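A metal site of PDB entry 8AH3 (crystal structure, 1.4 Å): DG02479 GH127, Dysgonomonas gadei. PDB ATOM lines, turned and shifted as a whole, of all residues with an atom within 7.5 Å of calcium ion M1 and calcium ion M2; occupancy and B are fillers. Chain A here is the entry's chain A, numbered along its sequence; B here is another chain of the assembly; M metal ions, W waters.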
ATOM      1  N   SER A  27       6.011  -8.108  21.314  1.00  0.00           N
ATOM      2  CA  SER A  27       5.395  -7.018  20.579  1.00  0.00           C
ATOM      3  C   SER A  27       6.408  -6.258  19.706  1.00  0.00           C
ATOM      4  O   SER A  27       6.124  -5.175  19.217  1.00  0.00           O
ATOM      5  CB  SER A  27       4.589  -6.156  21.547  1.00  0.00           C
ATOM      6  OG  SER A  27       5.408  -5.609  22.570  1.00  0.00           O
ATOM      7  N   ASN A  28       7.631  -6.792  19.477  1.00  0.00           N
ATOM      8  CA  ASN A  28       8.582  -6.138  18.592  1.00  0.00           C
ATOM      9  C   ASN A  28       7.927  -5.706  17.262  1.00  0.00           C
ATOM     10  O   ASN A  28       7.158  -6.459  16.690  1.00  0.00           O
ATOM     11  CB  ASN A  28       9.749  -7.067  18.295  1.00  0.00           C
ATOM     12  CG  ASN A  28      10.777  -6.474  17.384  1.00  0.00           C
ATOM     13  OD1 ASN A  28      11.685  -5.729  17.801  1.00  0.00           O
ATOM     14  ND2 ASN A  28      10.638  -6.826  16.123  1.00  0.00           N
ATOM     15  N   ASP A  29       8.279  -4.495  16.795  1.00  0.00           N
ATOM     16  CA  ASP A  29       7.763  -3.933  15.539  1.00  0.00           C
ATOM     17  C   ASP A  29       8.452  -4.659  14.385  1.00  0.00           C
ATOM     18  O   ASP A  29       9.651  -4.484  14.170  1.00  0.00           O
ATOM     19  CB  ASP A  29       8.088  -2.435  15.473  1.00  0.00           C
ATOM     20  CG  ASP A  29       7.586  -1.702  14.221  1.00  0.00           C
ATOM     21  OD1 ASP A  29       7.207  -2.365  13.241  1.00  0.00           O
ATOM     22  OD2 ASP A  29       7.558  -0.450  14.269  1.00  0.00           O
ATOM     23  N   PRO A  30       7.743  -5.489  13.600  1.00  0.00           N
ATOM     24  CA  PRO A  30       8.410  -6.250  12.537  1.00  0.00           C
ATOM     25  C   PRO A  30       9.002  -5.371  11.418  1.00  0.00           C
ATOM     26  O   PRO A  30       9.965  -5.782  10.785  1.00  0.00           O
ATOM     27  CB  PRO A  30       7.325  -7.217  12.055  1.00  0.00           C
ATOM     28  CG  PRO A  30       6.013  -6.554  12.412  1.00  0.00           C
ATOM     29  CD  PRO A  30       6.292  -5.784  13.694  1.00  0.00           C
ATOM     30  N   ALA A  31       8.506  -4.128  11.268  1.00  0.00           N
ATOM     31  CA  ALA A  31       9.049  -3.212  10.272  1.00  0.00           C
ATOM     32  C   ALA A  31      10.344  -2.558  10.740  1.00  0.00           C
ATOM     33  O   ALA A  31      10.924  -1.758  10.005  1.00  0.00           O
ATOM     34  CB  ALA A  31       8.019  -2.170   9.887  1.00  0.00           C
ATOM     35  N   GLY A  32      10.805  -2.807  12.004  1.00  0.00           N
ATOM     36  CA  GLY A  32      12.056  -2.236  12.429  1.00  0.00           C
ATOM     37  C   GLY A  32      11.942  -0.926  13.226  1.00  0.00           C
ATOM     38  O   GLY A  32      12.965  -0.342  13.577  1.00  0.00           O
ATOM     39  N   GLY A  33      10.717  -0.477  13.455  1.00  0.00           N
ATOM     40  CA  GLY A  33      10.532   0.876  13.954  1.00  0.00           C
ATOM     41  C   GLY A  33      10.270   0.895  15.470  1.00  0.00           C
ATOM     42  O   GLY A  33      10.707  -0.002  16.202  1.00  0.00           O
ATOM     43  N   VAL A  34       9.508   1.910  15.892  1.00  0.00           N
ATOM     44  CA  VAL A  34       9.343   2.242  17.300  1.00  0.00           C
ATOM     45  C   VAL A  34       8.058   1.656  17.830  1.00  0.00           C
ATOM     46  O   VAL A  34       7.808   1.754  19.050  1.00  0.00           O
ATOM     47  CB  VAL A  34       9.341   3.780  17.531  1.00  0.00           C
ATOM     48  CG1 VAL A  34      10.629   4.404  17.127  1.00  0.00           C
ATOM     49  CG2 VAL A  34       8.117   4.459  16.881  1.00  0.00           C
ATOM     50  N   LEU A  35       7.213   1.030  16.990  1.00  0.00           N
ATOM     51  CA  LEU A  35       5.910   0.549  17.435  1.00  0.00           C
ATOM     52  C   LEU A  35       6.048  -0.868  18.023  1.00  0.00           C
ATOM     53  O   LEU A  35       5.459  -1.843  17.531  1.00  0.00           O
ATOM     54  CB  LEU A  35       4.872   0.549  16.315  1.00  0.00           C
ATOM     55  CG  LEU A  35       4.530   1.926  15.716  1.00  0.00           C
ATOM     56  CD1 LEU A  35       3.534   1.755  14.573  1.00  0.00           C
ATOM     57  CD2 LEU A  35       3.980   2.853  16.784  1.00  0.00           C
ATOM     58  N   ASP A  36       6.849  -0.946  19.086  1.00  0.00           N
ATOM     59  CA  ASP A  36       7.226  -2.209  19.727  1.00  0.00           C
ATOM     60  C   ASP A  36       6.213  -2.656  20.764  1.00  0.00           C
ATOM     61  O   ASP A  36       6.566  -3.309  21.746  1.00  0.00           O
ATOM     62  CB  ASP A  36       8.632  -2.062  20.313  1.00  0.00           C
ATOM     63  CG  ASP A  36       9.733  -1.827  19.315  1.00  0.00           C
ATOM     64  OD1 ASP A  36       9.764  -2.570  18.243  1.00  0.00           O
ATOM     65  OD2 ASP A  36      10.577  -0.962  19.543  1.00  0.00           O
ATOM     66  N   TYR A 152       2.816  -3.862  25.810  1.00  0.00           N
ATOM     67  CA  TYR A 152       4.157  -4.367  25.522  1.00  0.00           C
ATOM     68  C   TYR A 152       4.293  -5.716  26.212  1.00  0.00           C
ATOM     69  O   TYR A 152       3.819  -5.889  27.348  1.00  0.00           O
ATOM     70  CB  TYR A 152       5.217  -3.453  26.141  1.00  0.00           C
ATOM     71  CG  TYR A 152       5.486  -2.132  25.476  1.00  0.00           C
ATOM     72  CD1 TYR A 152       4.683  -1.027  25.734  1.00  0.00           C
ATOM     73  CD2 TYR A 152       6.573  -1.974  24.654  1.00  0.00           C
ATOM     74  CE1 TYR A 152       4.971   0.207  25.194  1.00  0.00           C
ATOM     75  CE2 TYR A 152       6.876  -0.743  24.094  1.00  0.00           C
ATOM     76  CZ  TYR A 152       6.027   0.317  24.323  1.00  0.00           C
ATOM     77  OH  TYR A 152       6.364   1.499  23.786  1.00  0.00           O
ATOM     78  N   GLU B 188      16.356  10.101  18.875  1.00  0.00           N
ATOM     79  CA  GLU B 188      15.533   9.437  19.866  1.00  0.00           C
ATOM     80  C   GLU B 188      14.267  10.228  20.173  1.00  0.00           C
ATOM     81  O   GLU B 188      14.322  11.480  20.263  1.00  0.00           O
ATOM     82  CB  GLU B 188      16.308   9.260  21.159  1.00  0.00           C
ATOM     83  CG  GLU B 188      15.609   8.308  22.113  1.00  0.00           C
ATOM     84  CD  GLU B 188      15.345   6.979  21.389  1.00  0.00           C
ATOM     85  OE1 GLU B 188      16.329   6.202  21.314  1.00  0.00           O
ATOM     86  OE2 GLU B 188      14.197   6.758  20.960  1.00  0.00           O
ATOM     87  N   ASN B 197      14.168   3.072  10.596  1.00  0.00           N
ATOM     88  CA  ASN B 197      13.961   1.677  10.952  1.00  0.00           C
ATOM     89  C   ASN B 197      15.306   0.938  11.092  1.00  0.00           C
ATOM     90  O   ASN B 197      16.349   1.316  10.564  1.00  0.00           O
ATOM     91  CB  ASN B 197      13.089   0.971   9.920  1.00  0.00           C
ATOM     92  CG  ASN B 197      11.665   1.470   9.865  1.00  0.00           C
ATOM     93  OD1 ASN B 197      11.026   1.726  10.883  1.00  0.00           O
ATOM     94  ND2 ASN B 197      11.146   1.619   8.659  1.00  0.00           N
ATOM     95  N   ASN B 198      15.264  -0.209  11.816  1.00  0.00           N
ATOM     96  CA  ASN B 198      16.412  -1.096  11.948  1.00  0.00           C
ATOM     97  C   ASN B 198      15.872  -2.528  11.887  1.00  0.00           C
ATOM     98  O   ASN B 198      15.437  -3.092  12.903  1.00  0.00           O
ATOM     99  CB  ASN B 198      17.126  -0.875  13.282  1.00  0.00           C
ATOM    100  CG  ASN B 198      18.191  -1.909  13.568  1.00  0.00           C
ATOM    101  OD1 ASN B 198      18.770  -2.478  12.634  1.00  0.00           O
ATOM    102  ND2 ASN B 198      18.506  -2.108  14.847  1.00  0.00           N
ATOM    103  N   GLY B 232      17.225   4.101  26.629  1.00  0.00           N
ATOM    104  CA  GLY B 232      16.890   2.690  26.660  1.00  0.00           C
ATOM    105  C   GLY B 232      15.787   2.225  25.718  1.00  0.00           C
ATOM    106  O   GLY B 232      15.149   1.189  25.983  1.00  0.00           O
ATOM    107  N   GLU B 233      15.560   2.935  24.603  1.00  0.00           N
ATOM    108  CA  GLU B 233      14.527   2.502  23.670  1.00  0.00           C
ATOM    109  C   GLU B 233      15.009   1.302  22.809  1.00  0.00           C
ATOM    110  O   GLU B 233      14.181   0.679  22.162  1.00  0.00           O
ATOM    111  CB  GLU B 233      14.082   3.606  22.697  1.00  0.00           C
ATOM    112  CG  GLU B 233      13.333   4.748  23.380  1.00  0.00           C
ATOM    113  CD  GLU B 233      11.941   4.484  23.919  1.00  0.00           C
ATOM    114  OE1 GLU B 233      11.271   3.531  23.470  1.00  0.00           O
ATOM    115  OE2 GLU B 233      11.501   5.243  24.851  1.00  0.00           O
ATOM    116  N   GLY B 234      16.270   0.970  22.876  1.00  0.00           N
ATOM    117  CA  GLY B 234      16.834  -0.048  21.997  1.00  0.00           C
ATOM    118  C   GLY B 234      16.404  -1.482  22.336  1.00  0.00           C
ATOM    119  O   GLY B 234      16.413  -1.899  23.488  1.00  0.00           O
ATOM    120  N   ASP B 235      16.116  -2.268  21.299  1.00  0.00           N
ATOM    121  CA  ASP B 235      15.643  -3.638  21.399  1.00  0.00           C
ATOM    122  C   ASP B 235      16.802  -4.635  21.426  1.00  0.00           C
ATOM    123  O   ASP B 235      17.794  -4.459  20.741  1.00  0.00           O
ATOM    124  CB  ASP B 235      14.845  -3.988  20.138  1.00  0.00           C
ATOM    125  CG  ASP B 235      13.679  -3.049  19.834  1.00  0.00           C
ATOM    126  OD1 ASP B 235      13.265  -2.270  20.747  1.00  0.00           O
ATOM    127  OD2 ASP B 235      13.130  -3.127  18.686  1.00  0.00           O
ATOM    128  N   ASP B 236      16.626  -5.703  22.202  1.00  0.00           N
ATOM    129  CA  ASP B 236      17.553  -6.831  22.197  1.00  0.00           C
ATOM    130  C   ASP B 236      17.218  -7.742  21.000  1.00  0.00           C
ATOM    131  O   ASP B 236      16.059  -7.945  20.664  1.00  0.00           O
ATOM    132  CB  ASP B 236      17.489  -7.577  23.533  1.00  0.00           C
ATOM    133  CG  ASP B 236      16.123  -7.994  23.943  1.00  0.00           C
ATOM    134  OD1 ASP B 236      15.282  -7.097  24.122  1.00  0.00           O
ATOM    135  OD2 ASP B 236      15.885  -9.244  24.104  1.00  0.00           O
ATOM    136  N   PHE B 237      18.273  -8.290  20.404  1.00  0.00           N
ATOM    137  CA  PHE B 237      18.246  -9.245  19.290  1.00  0.00           C
ATOM    138  C   PHE B 237      19.135 -10.440  19.690  1.00  0.00           C
ATOM    139  O   PHE B 237      20.283 -10.255  20.072  1.00  0.00           O
ATOM    140  CB  PHE B 237      18.923  -8.644  18.041  1.00  0.00           C
ATOM    141  CG  PHE B 237      18.176  -7.615  17.248  1.00  0.00           C
ATOM    142  CD1 PHE B 237      17.752  -6.423  17.823  1.00  0.00           C
ATOM    143  CD2 PHE B 237      18.081  -7.719  15.874  1.00  0.00           C
ATOM    144  CE1 PHE B 237      17.091  -5.443  17.089  1.00  0.00           C
ATOM    145  CE2 PHE B 237      17.464  -6.724  15.135  1.00  0.00           C
ATOM    146  CZ  PHE B 237      17.003  -5.573  15.728  1.00  0.00           C
ATOM    147  N   GLY B 250      13.324  -8.219  21.181  1.00  0.00           N
ATOM    148  CA  GLY B 250      12.746  -7.475  22.304  1.00  0.00           C
ATOM    149  C   GLY B 250      12.120  -6.159  21.851  1.00  0.00           C
ATOM    150  O   GLY B 250      11.958  -5.891  20.670  1.00  0.00           O
ATOM    151  N   THR B 251      11.834  -5.294  22.841  1.00  0.00           N
ATOM    152  CA  THR B 251      11.043  -4.086  22.592  1.00  0.00           C
ATOM    153  C   THR B 251      11.738  -2.836  23.140  1.00  0.00           C
ATOM    154  O   THR B 251      11.373  -1.709  22.779  1.00  0.00           O
ATOM    155  CB  THR B 251       9.658  -4.236  23.199  1.00  0.00           C
ATOM    156  OG1 THR B 251       9.755  -4.475  24.607  1.00  0.00           O
ATOM    157  CG2 THR B 251       8.878  -5.370  22.587  1.00  0.00           C
ATOM    158  N   GLY B 252      12.712  -3.012  24.033  1.00  0.00           N
ATOM    159  CA  GLY B 252      13.374  -1.906  24.704  1.00  0.00           C
ATOM    160  C   GLY B 252      14.359  -2.457  25.718  1.00  0.00           C
ATOM    161  O   GLY B 252      14.385  -3.657  25.987  1.00  0.00           O
ATOM    162  N   THR B 253      15.205  -1.564  26.243  1.00  0.00           N
ATOM    163  CA  THR B 253      16.275  -1.969  27.137  1.00  0.00           C
ATOM    164  C   THR B 253      15.780  -2.180  28.572  1.00  0.00           C
ATOM    165  O   THR B 253      16.084  -3.206  29.199  1.00  0.00           O
ATOM    166  CB  THR B 253      17.431  -0.974  27.064  1.00  0.00           C
ATOM    167  OG1 THR B 253      17.874  -1.002  25.688  1.00  0.00           O
ATOM    168  CG2 THR B 253      18.546  -1.279  28.041  1.00  0.00           C
ATOM    169  N   GLU B 254      14.962  -1.257  29.087  1.00  0.00           N
ATOM    170  CA  GLU B 254      14.372  -1.502  30.397  1.00  0.00           C
ATOM    171  C   GLU B 254      13.522  -2.775  30.319  1.00  0.00           C
ATOM    172  O   GLU B 254      13.446  -3.561  31.273  1.00  0.00           O
ATOM    173  CB  GLU B 254      13.623  -0.257  30.921  1.00  0.00           C
ATOM    174  CG  GLU B 254      12.214  -0.007  30.389  1.00  0.00           C
ATOM    175  CD  GLU B 254      12.103   0.717  29.055  1.00  0.00           C
ATOM    176  OE1 GLU B 254      12.782   0.304  28.064  1.00  0.00           O
ATOM    177  OE2 GLU B 254      11.365   1.733  28.987  1.00  0.00           O
ATOM    178  N   ASP B 255      12.845  -2.990  29.173  1.00  0.00           N
ATOM    179  CA  ASP B 255      11.963  -4.123  28.943  1.00  0.00           C
ATOM    180  C   ASP B 255      12.733  -5.452  29.052  1.00  0.00           C
ATOM    181  O   ASP B 255      12.283  -6.379  29.748  1.00  0.00           O
ATOM    182  CB  ASP B 255      11.268  -3.967  27.573  1.00  0.00           C
ATOM    183  CG  ASP B 255      10.531  -2.648  27.325  1.00  0.00           C
ATOM    184  OD1 ASP B 255      10.335  -1.850  28.279  1.00  0.00           O
ATOM    185  OD2 ASP B 255      10.105  -2.417  26.173  1.00  0.00           O
ATOM    186  N   GLU B 309      20.100  -2.603  20.441  1.00  0.00           N
ATOM    187  CA  GLU B 309      20.213  -1.287  19.823  1.00  0.00           C
ATOM    188  C   GLU B 309      20.718  -0.281  20.878  1.00  0.00           C
ATOM    189  O   GLU B 309      20.330  -0.387  22.050  1.00  0.00           O
ATOM    190  CB  GLU B 309      18.878  -0.836  19.309  1.00  0.00           C
ATOM    191  CG  GLU B 309      18.184  -1.732  18.326  1.00  0.00           C
ATOM    192  CD  GLU B 309      16.848  -1.159  17.914  1.00  0.00           C
ATOM    193  OE1 GLU B 309      16.002  -0.949  18.763  1.00  0.00           O
ATOM    194  OE2 GLU B 309      16.648  -0.894  16.678  1.00  0.00           O
ATOM    195  N   GLY B 311      19.998   3.110  21.700  1.00  0.00           N
ATOM    196  CA  GLY B 311      18.877   3.940  21.322  1.00  0.00           C
ATOM    197  C   GLY B 311      18.063   3.292  20.228  1.00  0.00           C
ATOM    198  O   GLY B 311      18.539   2.320  19.586  1.00  0.00           O
ATOM    199  N   HIS B 312      16.857   3.786  19.994  1.00  0.00           N
ATOM    200  CA  HIS B 312      16.034   3.274  18.907  1.00  0.00           C
ATOM    201  C   HIS B 312      16.797   3.364  17.581  1.00  0.00           C
ATOM    202  O   HIS B 312      17.410   4.390  17.251  1.00  0.00           O
ATOM    203  CB  HIS B 312      14.691   3.984  18.756  1.00  0.00           C
ATOM    204  CG  HIS B 312      14.037   3.550  17.488  1.00  0.00           C
ATOM    205  ND1 HIS B 312      13.486   2.285  17.322  1.00  0.00           N
ATOM    206  CD2 HIS B 312      14.047   4.162  16.274  1.00  0.00           C
ATOM    207  CE1 HIS B 312      13.133   2.143  16.034  1.00  0.00           C
ATOM    208  NE2 HIS B 312      13.489   3.298  15.370  1.00  0.00           N
ATOM    209  N   ALA B 313      16.856   2.203  16.860  1.00  0.00           N
ATOM    210  CA  ALA B 313      17.651   2.118  15.640  1.00  0.00           C
ATOM    211  C   ALA B 313      19.056   2.680  15.769  1.00  0.00           C
ATOM    212  O   ALA B 313      19.612   3.243  14.805  1.00  0.00           O
ATOM    213  CB  ALA B 313      16.915   2.816  14.502  1.00  0.00           C
HETATM  214 CA    CA M   1      11.918  -1.642  17.480  1.00  0.00          CA
HETATM  215 CA    CA M   2      12.222  -0.228  21.088  1.00  0.00          CA
HETATM  216  O   HOH W   1      11.834   2.018  20.097  1.00  0.00           O
HETATM  217  O   HOH W   2      13.888  -1.186  16.059  1.00  0.00           O
HETATM  218  O   HOH W   3      10.897   1.049  22.725  1.00  0.00           O
HETATM  219  O   HOH W   4      13.440  -0.039  18.824  1.00  0.00           O
HETATM  220  O   HOH W   5      11.657  -3.245  15.770  1.00  0.00           O
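Of the 30 residues printed, 4 come within 4 Å of calcium ion M2.
Water W2 lies within hydrogen-bond range of O of Gly 32 and OE2 of Glu 309 of chain B.
Water W4 lies within hydrogen-bond range of the side-chain carboxylate (OE1) of Glu 309 of chain B and a ring nitrogen (ND1) of His 312 of chain B.
Water W5 bridges O of Asp 29 (2.8 Å) and OD1 of Asn 28 (3.2 Å).
Calcium ion M1 is bound by the side-chain carboxylate (OD2) of Asp 235 of chain B, water W5, the backbone carbonyl oxygen (O) of Gly 33, the side-chain carboxylate (OD1) of Asp 36, water W2, the side-chain carboxylate (OD2) of Asp 36 and water W4.
The side-chain carboxylate (OD2) of Asp 235 of chain B lies close to the side-chain amide oxygen (OD1) of Asn 28 (3.1 Å).
N of Asp 235 of chain B is in hydrogen-bond range of OE1 of Glu 309 of chain B (2.9 Å).
The backbone NH (N) of Gly 33 lies close to the side-chain amide oxygen (OD1) of Asn 197 of chain B, 3.4 Å away.
The side-chain carboxylate (OD2) of Asp 29 sits close to the backbone NH (N) of Gly 33.
The backbone NH of Asp 29 lies close to the side-chain carboxylate of Asp 36, at 2.8 Å.
The backbone carbonyl oxygen (O) of Asp 36 lies within hydrogen-bond range of the side-chain hydroxyl (OG) of Ser 27 (2.7 Å).
OG1 of Thr 251 of chain B is in hydrogen-bond range of OD2 of Asp 255 of chain B, at 2.6 Å.
The backbone NH (N) of Gly 252 of chain B lies close to the side-chain carboxylate (OD1) of Asp 235 of chain B, 3.4 Å away.
Calcium ion M2 is bound by the side-chain carboxylate of Asp 235 of chain B (2.3 Å), the side-chain carboxylate of Asp 36 (2.4 Å), the backbone carbonyl oxygen of Thr 251 of chain B (2.4 Å), the backbone carbonyl oxygen of Glu 233 of chain B (2.4 Å), water W3 (2.5 Å), water W1 (2.5 Å) and water W4 (2.6 Å).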
